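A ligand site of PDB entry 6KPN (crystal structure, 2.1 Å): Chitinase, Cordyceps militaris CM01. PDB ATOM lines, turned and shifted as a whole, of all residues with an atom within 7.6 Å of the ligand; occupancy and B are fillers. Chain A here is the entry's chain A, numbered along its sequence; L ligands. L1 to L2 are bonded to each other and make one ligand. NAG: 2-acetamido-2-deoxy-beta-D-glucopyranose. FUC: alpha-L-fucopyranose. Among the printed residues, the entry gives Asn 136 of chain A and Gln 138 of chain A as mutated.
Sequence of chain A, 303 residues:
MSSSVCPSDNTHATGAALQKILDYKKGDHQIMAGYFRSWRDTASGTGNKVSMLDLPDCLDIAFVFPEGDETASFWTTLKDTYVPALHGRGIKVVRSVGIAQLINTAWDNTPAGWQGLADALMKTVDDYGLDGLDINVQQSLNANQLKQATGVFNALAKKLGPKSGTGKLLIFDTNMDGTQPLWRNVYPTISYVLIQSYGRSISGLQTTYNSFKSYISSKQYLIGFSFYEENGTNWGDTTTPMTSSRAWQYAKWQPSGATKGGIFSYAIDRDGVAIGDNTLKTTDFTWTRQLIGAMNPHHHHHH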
ATOM      1  N   PHE A  65      38.416  29.573 -17.637  1.00  0.00           N
ATOM      2  CA  PHE A  65      37.919  30.646 -18.524  1.00  0.00           C
ATOM      3  C   PHE A  65      37.564  31.823 -17.619  1.00  0.00           C
ATOM      4  O   PHE A  65      36.512  31.853 -16.999  1.00  0.00           O
ATOM      5  CB  PHE A  65      36.739  30.145 -19.367  1.00  0.00           C
ATOM      6  CG  PHE A  65      36.333  31.060 -20.488  1.00  0.00           C
ATOM      7  CD1 PHE A  65      35.409  32.066 -20.284  1.00  0.00           C
ATOM      8  CD2 PHE A  65      36.856  30.884 -21.759  1.00  0.00           C
ATOM      9  CE1 PHE A  65      35.075  32.930 -21.314  1.00  0.00           C
ATOM     10  CE2 PHE A  65      36.504  31.732 -22.812  1.00  0.00           C
ATOM     11  CZ  PHE A  65      35.613  32.757 -22.577  1.00  0.00           C
ATOM     12  N   ASN A 136      40.726  31.085 -28.123  1.00  0.00           N
ATOM     13  CA  ASN A 136      39.330  31.215 -28.589  1.00  0.00           C
ATOM     14  C   ASN A 136      39.292  32.196 -29.768  1.00  0.00           C
ATOM     15  O   ASN A 136      39.478  33.447 -29.561  1.00  0.00           O
ATOM     16  CB  ASN A 136      38.397  31.613 -27.448  1.00  0.00           C
ATOM     17  CG  ASN A 136      36.937  31.689 -27.889  1.00  0.00           C
ATOM     18  OD1 ASN A 136      36.642  31.707 -29.062  1.00  0.00           O
ATOM     19  ND2 ASN A 136      36.030  31.689 -26.930  1.00  0.00           N
ATOM     20  N   GLN A 138      36.924  33.799 -32.771  1.00  0.00           N
ATOM     21  CA  GLN A 138      35.504  34.068 -33.156  1.00  0.00           C
ATOM     22  C   GLN A 138      35.458  35.301 -34.042  1.00  0.00           C
ATOM     23  O   GLN A 138      34.458  36.036 -34.010  1.00  0.00           O
ATOM     24  CB  GLN A 138      34.642  34.246 -31.913  1.00  0.00           C
ATOM     25  CG  GLN A 138      34.567  33.012 -31.014  1.00  0.00           C
ATOM     26  CD  GLN A 138      33.654  33.243 -29.842  1.00  0.00           C
ATOM     27  OE1 GLN A 138      33.541  34.361 -29.341  1.00  0.00           O
ATOM     28  NE2 GLN A 138      32.982  32.211 -29.366  1.00  0.00           N
ATOM     29  N   THR A 174      36.955  27.392 -31.685  1.00  0.00           N
ATOM     30  CA  THR A 174      36.445  28.371 -32.676  1.00  0.00           C
ATOM     31  C   THR A 174      34.973  28.104 -33.020  1.00  0.00           C
ATOM     32  O   THR A 174      34.435  26.993 -32.808  1.00  0.00           O
ATOM     33  CB  THR A 174      37.406  28.403 -33.876  1.00  0.00           C
ATOM     34  OG1 THR A 174      37.083  29.487 -34.756  1.00  0.00           O
ATOM     35  CG2 THR A 174      37.386  27.091 -34.640  1.00  0.00           C
ATOM     36  N   ASN A 175      34.332  29.133 -33.551  1.00  0.00           N
ATOM     37  CA  ASN A 175      32.967  29.030 -34.093  1.00  0.00           C
ATOM     38  C   ASN A 175      33.039  29.269 -35.602  1.00  0.00           C
ATOM     39  O   ASN A 175      31.976  29.489 -36.228  1.00  0.00           O
ATOM     40  CB  ASN A 175      32.059  29.971 -33.319  1.00  0.00           C
ATOM     41  CG  ASN A 175      32.347  31.430 -33.592  1.00  0.00           C
ATOM     42  OD1 ASN A 175      33.339  31.747 -34.242  1.00  0.00           O
ATOM     43  ND2 ASN A 175      31.433  32.291 -33.178  1.00  0.00           N
ATOM     44  N   MET A 176      34.251  29.259 -36.192  1.00  0.00           N
ATOM     45  CA  MET A 176      34.453  29.400 -37.662  1.00  0.00           C
ATOM     46  C   MET A 176      34.984  28.076 -38.235  1.00  0.00           C
ATOM     47  O   MET A 176      35.007  27.059 -37.498  1.00  0.00           O
ATOM     48  CB  MET A 176      35.371  30.589 -37.947  1.00  0.00           C
ATOM     49  CG  MET A 176      34.737  31.908 -37.559  1.00  0.00           C
ATOM     50  SD  MET A 176      35.881  33.320 -37.517  1.00  0.00           S
ATOM     51  CE  MET A 176      35.951  33.644 -39.279  1.00  0.00           C
ATOM     52  N   ILE A 195      35.158  22.870 -31.884  1.00  0.00           N
ATOM     53  CA  ILE A 195      34.144  23.686 -32.637  1.00  0.00           C
ATOM     54  C   ILE A 195      32.966  23.997 -31.712  1.00  0.00           C
ATOM     55  O   ILE A 195      32.222  23.078 -31.360  1.00  0.00           O
ATOM     56  CB  ILE A 195      33.724  23.048 -33.960  1.00  0.00           C
ATOM     57  CG1 ILE A 195      34.930  22.453 -34.697  1.00  0.00           C
ATOM     58  CG2 ILE A 195      33.019  24.055 -34.838  1.00  0.00           C
ATOM     59  CD1 ILE A 195      36.007  23.471 -35.019  1.00  0.00           C
ATOM     60  N   GLN A 196      32.883  25.257 -31.299  1.00  0.00           N
ATOM     61  CA  GLN A 196      31.688  25.875 -30.686  1.00  0.00           C
ATOM     62  C   GLN A 196      30.529  25.641 -31.654  1.00  0.00           C
ATOM     63  O   GLN A 196      30.529  26.242 -32.752  1.00  0.00           O
ATOM     64  CB  GLN A 196      31.918  27.373 -30.433  1.00  0.00           C
ATOM     65  CG  GLN A 196      33.010  27.718 -29.418  1.00  0.00           C
ATOM     66  CD  GLN A 196      33.463  29.140 -29.662  1.00  0.00           C
ATOM     67  OE1 GLN A 196      32.636  30.003 -29.948  1.00  0.00           O
ATOM     68  NE2 GLN A 196      34.764  29.403 -29.660  1.00  0.00           N
ATOM     69  N   SER A 197      29.598  24.781 -31.249  1.00  0.00           N
ATOM     70  CA  SER A 197      28.477  24.318 -32.113  1.00  0.00           C
ATOM     71  C   SER A 197      27.119  24.530 -31.422  1.00  0.00           C
ATOM     72  O   SER A 197      26.186  23.705 -31.688  1.00  0.00           O
ATOM     73  CB  SER A 197      28.672  22.856 -32.493  1.00  0.00           C
ATOM     74  OG  SER A 197      29.838  22.666 -33.278  1.00  0.00           O
ATOM     75  N   TYR A 198      26.972  25.585 -30.611  1.00  0.00           N
ATOM     76  CA  TYR A 198      25.776  25.774 -29.747  1.00  0.00           C
ATOM     77  C   TYR A 198      24.559  26.039 -30.652  1.00  0.00           C
ATOM     78  O   TYR A 198      24.682  26.843 -31.593  1.00  0.00           O
ATOM     79  CB  TYR A 198      25.980  26.880 -28.693  1.00  0.00           C
ATOM     80  CG  TYR A 198      27.352  26.937 -28.051  1.00  0.00           C
ATOM     81  CD1 TYR A 198      28.102  25.785 -27.834  1.00  0.00           C
ATOM     82  CD2 TYR A 198      27.893  28.166 -27.657  1.00  0.00           C
ATOM     83  CE1 TYR A 198      29.377  25.842 -27.270  1.00  0.00           C
ATOM     84  CE2 TYR A 198      29.145  28.229 -27.066  1.00  0.00           C
ATOM     85  CZ  TYR A 198      29.890  27.072 -26.886  1.00  0.00           C
ATOM     86  OH  TYR A 198      31.115  27.155 -26.337  1.00  0.00           O
ATOM     87  N   GLY A 199      23.456  25.316 -30.416  1.00  0.00           N
ATOM     88  CA  GLY A 199      22.166  25.404 -31.132  1.00  0.00           C
ATOM     89  C   GLY A 199      22.265  25.113 -32.624  1.00  0.00           C
ATOM     90  O   GLY A 199      21.469  25.697 -33.380  1.00  0.00           O
ATOM     91  N   ARG A 200      23.186  24.259 -33.090  1.00  0.00           N
ATOM     92  CA  ARG A 200      23.440  24.023 -34.541  1.00  0.00           C
ATOM     93  C   ARG A 200      22.680  22.781 -35.031  1.00  0.00           C
ATOM     94  O   ARG A 200      22.288  21.960 -34.200  1.00  0.00           O
ATOM     95  CB  ARG A 200      24.938  23.846 -34.774  1.00  0.00           C
ATOM     96  CG  ARG A 200      25.740  25.139 -34.654  1.00  0.00           C
ATOM     97  CD  ARG A 200      27.073  25.121 -35.375  1.00  0.00           C
ATOM     98  NE  ARG A 200      27.802  26.360 -35.130  1.00  0.00           N
ATOM     99  CZ  ARG A 200      29.019  26.644 -35.584  1.00  0.00           C
ATOM    100  NH1 ARG A 200      29.678  25.755 -36.313  1.00  0.00           N
ATOM    101  NH2 ARG A 200      29.579  27.791 -35.270  1.00  0.00           N
ATOM    102  N   GLY A 224      31.171  21.186 -29.522  1.00  0.00           N
ATOM    103  CA  GLY A 224      30.766  21.892 -28.301  1.00  0.00           C
ATOM    104  C   GLY A 224      29.273  22.189 -28.286  1.00  0.00           C
ATOM    105  O   GLY A 224      28.745  22.781 -29.263  1.00  0.00           O
ATOM    106  N   PHE A 225      28.635  21.806 -27.180  1.00  0.00           N
ATOM    107  CA  PHE A 225      27.303  22.331 -26.758  1.00  0.00           C
ATOM    108  C   PHE A 225      27.494  23.255 -25.537  1.00  0.00           C
ATOM    109  O   PHE A 225      28.505  23.168 -24.776  1.00  0.00           O
ATOM    110  CB  PHE A 225      26.360  21.154 -26.493  1.00  0.00           C
ATOM    111  CG  PHE A 225      26.676  20.427 -25.211  1.00  0.00           C
ATOM    112  CD1 PHE A 225      27.634  19.433 -25.179  1.00  0.00           C
ATOM    113  CD2 PHE A 225      26.020  20.771 -24.034  1.00  0.00           C
ATOM    114  CE1 PHE A 225      27.929  18.776 -23.990  1.00  0.00           C
ATOM    115  CE2 PHE A 225      26.317  20.116 -22.862  1.00  0.00           C
ATOM    116  CZ  PHE A 225      27.276  19.122 -22.830  1.00  0.00           C
ATOM    117  N   SER A 226      26.512  24.129 -25.319  1.00  0.00           N
ATOM    118  CA  SER A 226      26.429  25.003 -24.119  1.00  0.00           C
ATOM    119  C   SER A 226      25.409  24.437 -23.119  1.00  0.00           C
ATOM    120  O   SER A 226      24.332  23.932 -23.555  1.00  0.00           O
ATOM    121  CB  SER A 226      26.098  26.426 -24.493  1.00  0.00           C
ATOM    122  OG  SER A 226      26.393  27.287 -23.402  1.00  0.00           O
ATOM    123  N   GLU A 229      23.287  29.226 -19.440  1.00  0.00           N
ATOM    124  CA  GLU A 229      23.873  30.318 -18.625  1.00  0.00           C
ATOM    125  C   GLU A 229      22.763  31.178 -18.025  1.00  0.00           C
ATOM    126  O   GLU A 229      21.895  31.622 -18.799  1.00  0.00           O
ATOM    127  CB  GLU A 229      24.785  31.200 -19.471  1.00  0.00           C
ATOM    128  CG  GLU A 229      26.183  30.609 -19.616  1.00  0.00           C
ATOM    129  CD  GLU A 229      27.112  31.562 -20.338  1.00  0.00           C
ATOM    130  OE1 GLU A 229      26.954  31.704 -21.605  1.00  0.00           O
ATOM    131  OE2 GLU A 229      27.992  32.181 -19.631  1.00  0.00           O
ATOM    132  N   THR A 233      21.936  33.417 -23.483  1.00  0.00           N
ATOM    133  CA  THR A 233      21.321  32.936 -24.734  1.00  0.00           C
ATOM    134  C   THR A 233      20.714  31.547 -24.477  1.00  0.00           C
ATOM    135  O   THR A 233      21.334  30.731 -23.725  1.00  0.00           O
ATOM    136  CB  THR A 233      22.340  32.887 -25.867  1.00  0.00           C
ATOM    137  OG1 THR A 233      22.806  34.231 -25.968  1.00  0.00           O
ATOM    138  CG2 THR A 233      21.749  32.417 -27.179  1.00  0.00           C
ATOM    139  N   TRP A 235      20.322  28.484 -26.179  1.00  0.00           N
ATOM    140  CA  TRP A 235      20.810  27.658 -27.329  1.00  0.00           C
ATOM    141  C   TRP A 235      19.970  26.381 -27.470  1.00  0.00           C
ATOM    142  O   TRP A 235      19.942  25.826 -28.563  1.00  0.00           O
ATOM    143  CB  TRP A 235      22.290  27.280 -27.163  1.00  0.00           C
ATOM    144  CG  TRP A 235      23.219  28.441 -27.167  1.00  0.00           C
ATOM    145  CD1 TRP A 235      23.871  28.942 -26.084  1.00  0.00           C
ATOM    146  CD2 TRP A 235      23.603  29.246 -28.278  1.00  0.00           C
ATOM    147  NE1 TRP A 235      24.603  30.036 -26.448  1.00  0.00           N
ATOM    148  CE2 TRP A 235      24.483  30.232 -27.790  1.00  0.00           C
ATOM    149  CE3 TRP A 235      23.289  29.243 -29.639  1.00  0.00           C
ATOM    150  CZ2 TRP A 235      25.045  31.216 -28.605  1.00  0.00           C
ATOM    151  CZ3 TRP A 235      23.836  30.208 -30.447  1.00  0.00           C
ATOM    152  CH2 TRP A 235      24.709  31.176 -29.939  1.00  0.00           C
ATOM    153  N   ASP A 237      20.512  23.369 -26.137  1.00  0.00           N
ATOM    154  CA  ASP A 237      21.415  22.209 -26.312  1.00  0.00           C
ATOM    155  C   ASP A 237      21.138  21.137 -25.260  1.00  0.00           C
ATOM    156  O   ASP A 237      21.641  20.004 -25.433  1.00  0.00           O
ATOM    157  CB  ASP A 237      22.889  22.644 -26.233  1.00  0.00           C
ATOM    158  CG  ASP A 237      23.418  23.529 -27.354  1.00  0.00           C
ATOM    159  OD1 ASP A 237      22.742  23.708 -28.362  1.00  0.00           O
ATOM    160  OD2 ASP A 237      24.526  24.049 -27.195  1.00  0.00           O
ATOM    161  N   TYR A 250      25.198  15.005 -30.064  1.00  0.00           N
ATOM    162  CA  TYR A 250      26.636  15.348 -30.225  1.00  0.00           C
ATOM    163  C   TYR A 250      27.486  14.173 -29.710  1.00  0.00           C
ATOM    164  O   TYR A 250      28.379  13.794 -30.436  1.00  0.00           O
ATOM    165  CB  TYR A 250      26.969  16.685 -29.539  1.00  0.00           C
ATOM    166  CG  TYR A 250      26.563  17.882 -30.355  1.00  0.00           C
ATOM    167  CD1 TYR A 250      25.743  17.766 -31.454  1.00  0.00           C
ATOM    168  CD2 TYR A 250      27.007  19.138 -30.024  1.00  0.00           C
ATOM    169  CE1 TYR A 250      25.388  18.859 -32.208  1.00  0.00           C
ATOM    170  CE2 TYR A 250      26.648  20.249 -30.752  1.00  0.00           C
ATOM    171  CZ  TYR A 250      25.831  20.119 -31.852  1.00  0.00           C
ATOM    172  OH  TYR A 250      25.452  21.211 -32.586  1.00  0.00           O
ATOM    173  N   PHE A 264      32.782  18.816 -25.918  1.00  0.00           N
ATOM    174  CA  PHE A 264      32.980  19.697 -24.755  1.00  0.00           C
ATOM    175  C   PHE A 264      31.681  20.450 -24.479  1.00  0.00           C
ATOM    176  O   PHE A 264      30.882  20.665 -25.411  1.00  0.00           O
ATOM    177  CB  PHE A 264      34.161  20.638 -25.009  1.00  0.00           C
ATOM    178  CG  PHE A 264      33.925  21.629 -26.114  1.00  0.00           C
ATOM    179  CD1 PHE A 264      34.219  21.300 -27.426  1.00  0.00           C
ATOM    180  CD2 PHE A 264      33.401  22.885 -25.844  1.00  0.00           C
ATOM    181  CE1 PHE A 264      34.028  22.226 -28.434  1.00  0.00           C
ATOM    182  CE2 PHE A 264      33.204  23.810 -26.864  1.00  0.00           C
ATOM    183  CZ  PHE A 264      33.523  23.477 -28.150  1.00  0.00           C
ATOM    184  N   TYR A 266      30.271  24.233 -22.827  1.00  0.00           N
ATOM    185  CA  TYR A 266      30.504  25.591 -22.281  1.00  0.00           C
ATOM    186  C   TYR A 266      29.691  25.746 -20.999  1.00  0.00           C
ATOM    187  O   TYR A 266      28.541  25.245 -20.955  1.00  0.00           O
ATOM    188  CB  TYR A 266      30.128  26.695 -23.253  1.00  0.00           C
ATOM    189  CG  TYR A 266      30.604  28.034 -22.741  1.00  0.00           C
ATOM    190  CD1 TYR A 266      31.955  28.371 -22.780  1.00  0.00           C
ATOM    191  CD2 TYR A 266      29.723  28.935 -22.146  1.00  0.00           C
ATOM    192  CE1 TYR A 266      32.402  29.588 -22.284  1.00  0.00           C
ATOM    193  CE2 TYR A 266      30.149  30.156 -21.664  1.00  0.00           C
ATOM    194  CZ  TYR A 266      31.496  30.472 -21.724  1.00  0.00           C
ATOM    195  OH  TYR A 266      31.925  31.657 -21.234  1.00  0.00           O
HETATM  196  C1  NAG L   1      27.915  34.486 -29.931  1.00  0.00           C
HETATM  197  C2  NAG L   1      28.263  35.413 -28.788  1.00  0.00           C
HETATM  198  C3  NAG L   1      29.595  34.948 -28.278  1.00  0.00           C
HETATM  199  C4  NAG L   1      29.522  33.492 -27.828  1.00  0.00           C
HETATM  200  C5  NAG L   1      29.100  32.653 -28.997  1.00  0.00           C
HETATM  201  C6  NAG L   1      28.979  31.148 -28.673  1.00  0.00           C
HETATM  202  C7  NAG L   1      27.454  37.756 -28.928  1.00  0.00           C
HETATM  203  C8  NAG L   1      27.690  39.022 -29.694  1.00  0.00           C
HETATM  204  N2  NAG L   1      28.355  36.791 -29.223  1.00  0.00           N
HETATM  205  O1  NAG L   1      26.615  34.714 -30.470  1.00  0.00           O
HETATM  206  O3  NAG L   1      29.844  35.878 -27.260  1.00  0.00           O
HETATM  207  O4  NAG L   1      30.777  32.956 -27.444  1.00  0.00           O
HETATM  208  O5  NAG L   1      27.858  33.189 -29.356  1.00  0.00           O
HETATM  209  O6  NAG L   1      28.407  30.381 -29.753  1.00  0.00           O
HETATM  210  O7  NAG L   1      26.480  37.651 -28.163  1.00  0.00           O
HETATM  211  C1  FUC L   2      29.224  30.216 -30.941  1.00  0.00           C
HETATM  212  C2  FUC L   2      28.720  28.935 -31.590  1.00  0.00           C
HETATM  213  C3  FUC L   2      27.319  29.102 -32.204  1.00  0.00           C
HETATM  214  C4  FUC L   2      27.345  30.248 -33.205  1.00  0.00           C
HETATM  215  C5  FUC L   2      27.866  31.503 -32.492  1.00  0.00           C
HETATM  216  C6  FUC L   2      27.897  32.642 -33.487  1.00  0.00           C
HETATM  217  O2  FUC L   2      28.638  27.983 -30.541  1.00  0.00           O
HETATM  218  O3  FUC L   2      26.864  27.913 -32.840  1.00  0.00           O
HETATM  219  O4  FUC L   2      28.154  29.862 -34.331  1.00  0.00           O
HETATM  220  O5  FUC L   2      29.191  31.277 -31.903  1.00  0.00           O
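The backbone carbonyl oxygen (O) of Asn 175 lies within hydrogen-bond range of the guanidinium group (NH2) of Arg 200 (3.1 Å).
N of Ser 197 is in hydrogen-bond range of O of Gly 224, at 2.9 Å.
The side-chain amide nitrogen (NE2) of Gln 196 sits close to the side-chain amide nitrogen (NE2) of Gln 138, at 3.3 Å.
The side-chain hydroxyl of Ser 197 lies within hydrogen-bond range of the backbone carbonyl oxygen of Ile 195.
The guanidinium group (NH2) of Arg 200 lies within hydrogen-bond range of the backbone carbonyl oxygen (O) of Gln 196 (3.1 Å).
OD1 of Asn 136 sits at hydrogen-bond distance from NE2 of Gln 196, 3.0 Å away.
The backbone carbonyl oxygen (O) of Thr 174 lies within hydrogen-bond range of the backbone NH (N) of Gln 196, at 2.8 Å.
O of Ser 197 is in hydrogen-bond range of OH of Tyr 250, 2.8 Å away.
NE2 of Gln 138 lies within hydrogen-bond range of O4 of NAG L1.
O of Tyr 198 sits at hydrogen-bond distance from O3 of FUC L2.
The backbone NH (N) of Tyr 198 lies within hydrogen-bond range of an oxygen (O2) of FUC L2.
The backbone carbonyl oxygen (O) of Gln 196 lies close to an oxygen (O2) of FUC L2 (3.4 Å).
An oxygen (O5) of FUC L2 sits at hydrogen-bond distance from the side-chain amide nitrogen of Asn 175, 2.8 Å away.
N of Ser 197 lies within hydrogen-bond range of O2 of FUC L2 (3.4 Å).
The guanidinium group (NH2) of Arg 200 lies within hydrogen-bond range of an oxygen (O4) of FUC L2 (2.7 Å).
CZ2 of Trp 235 touches O5 of NAG L1, at 3.5 Å.
Hydrophobic or aromatic side chains within 4 Å of the ligand: Tyr 198 and Trp 235.
Seven residues have an atom within 4 Å of the ligand: Gln 138, Asn 175, Gln 196, Ser 197, Tyr 198, Arg 200 and Trp 235.
Along chain A the residues within 4 Å of the ligand span positions 138 to 235.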
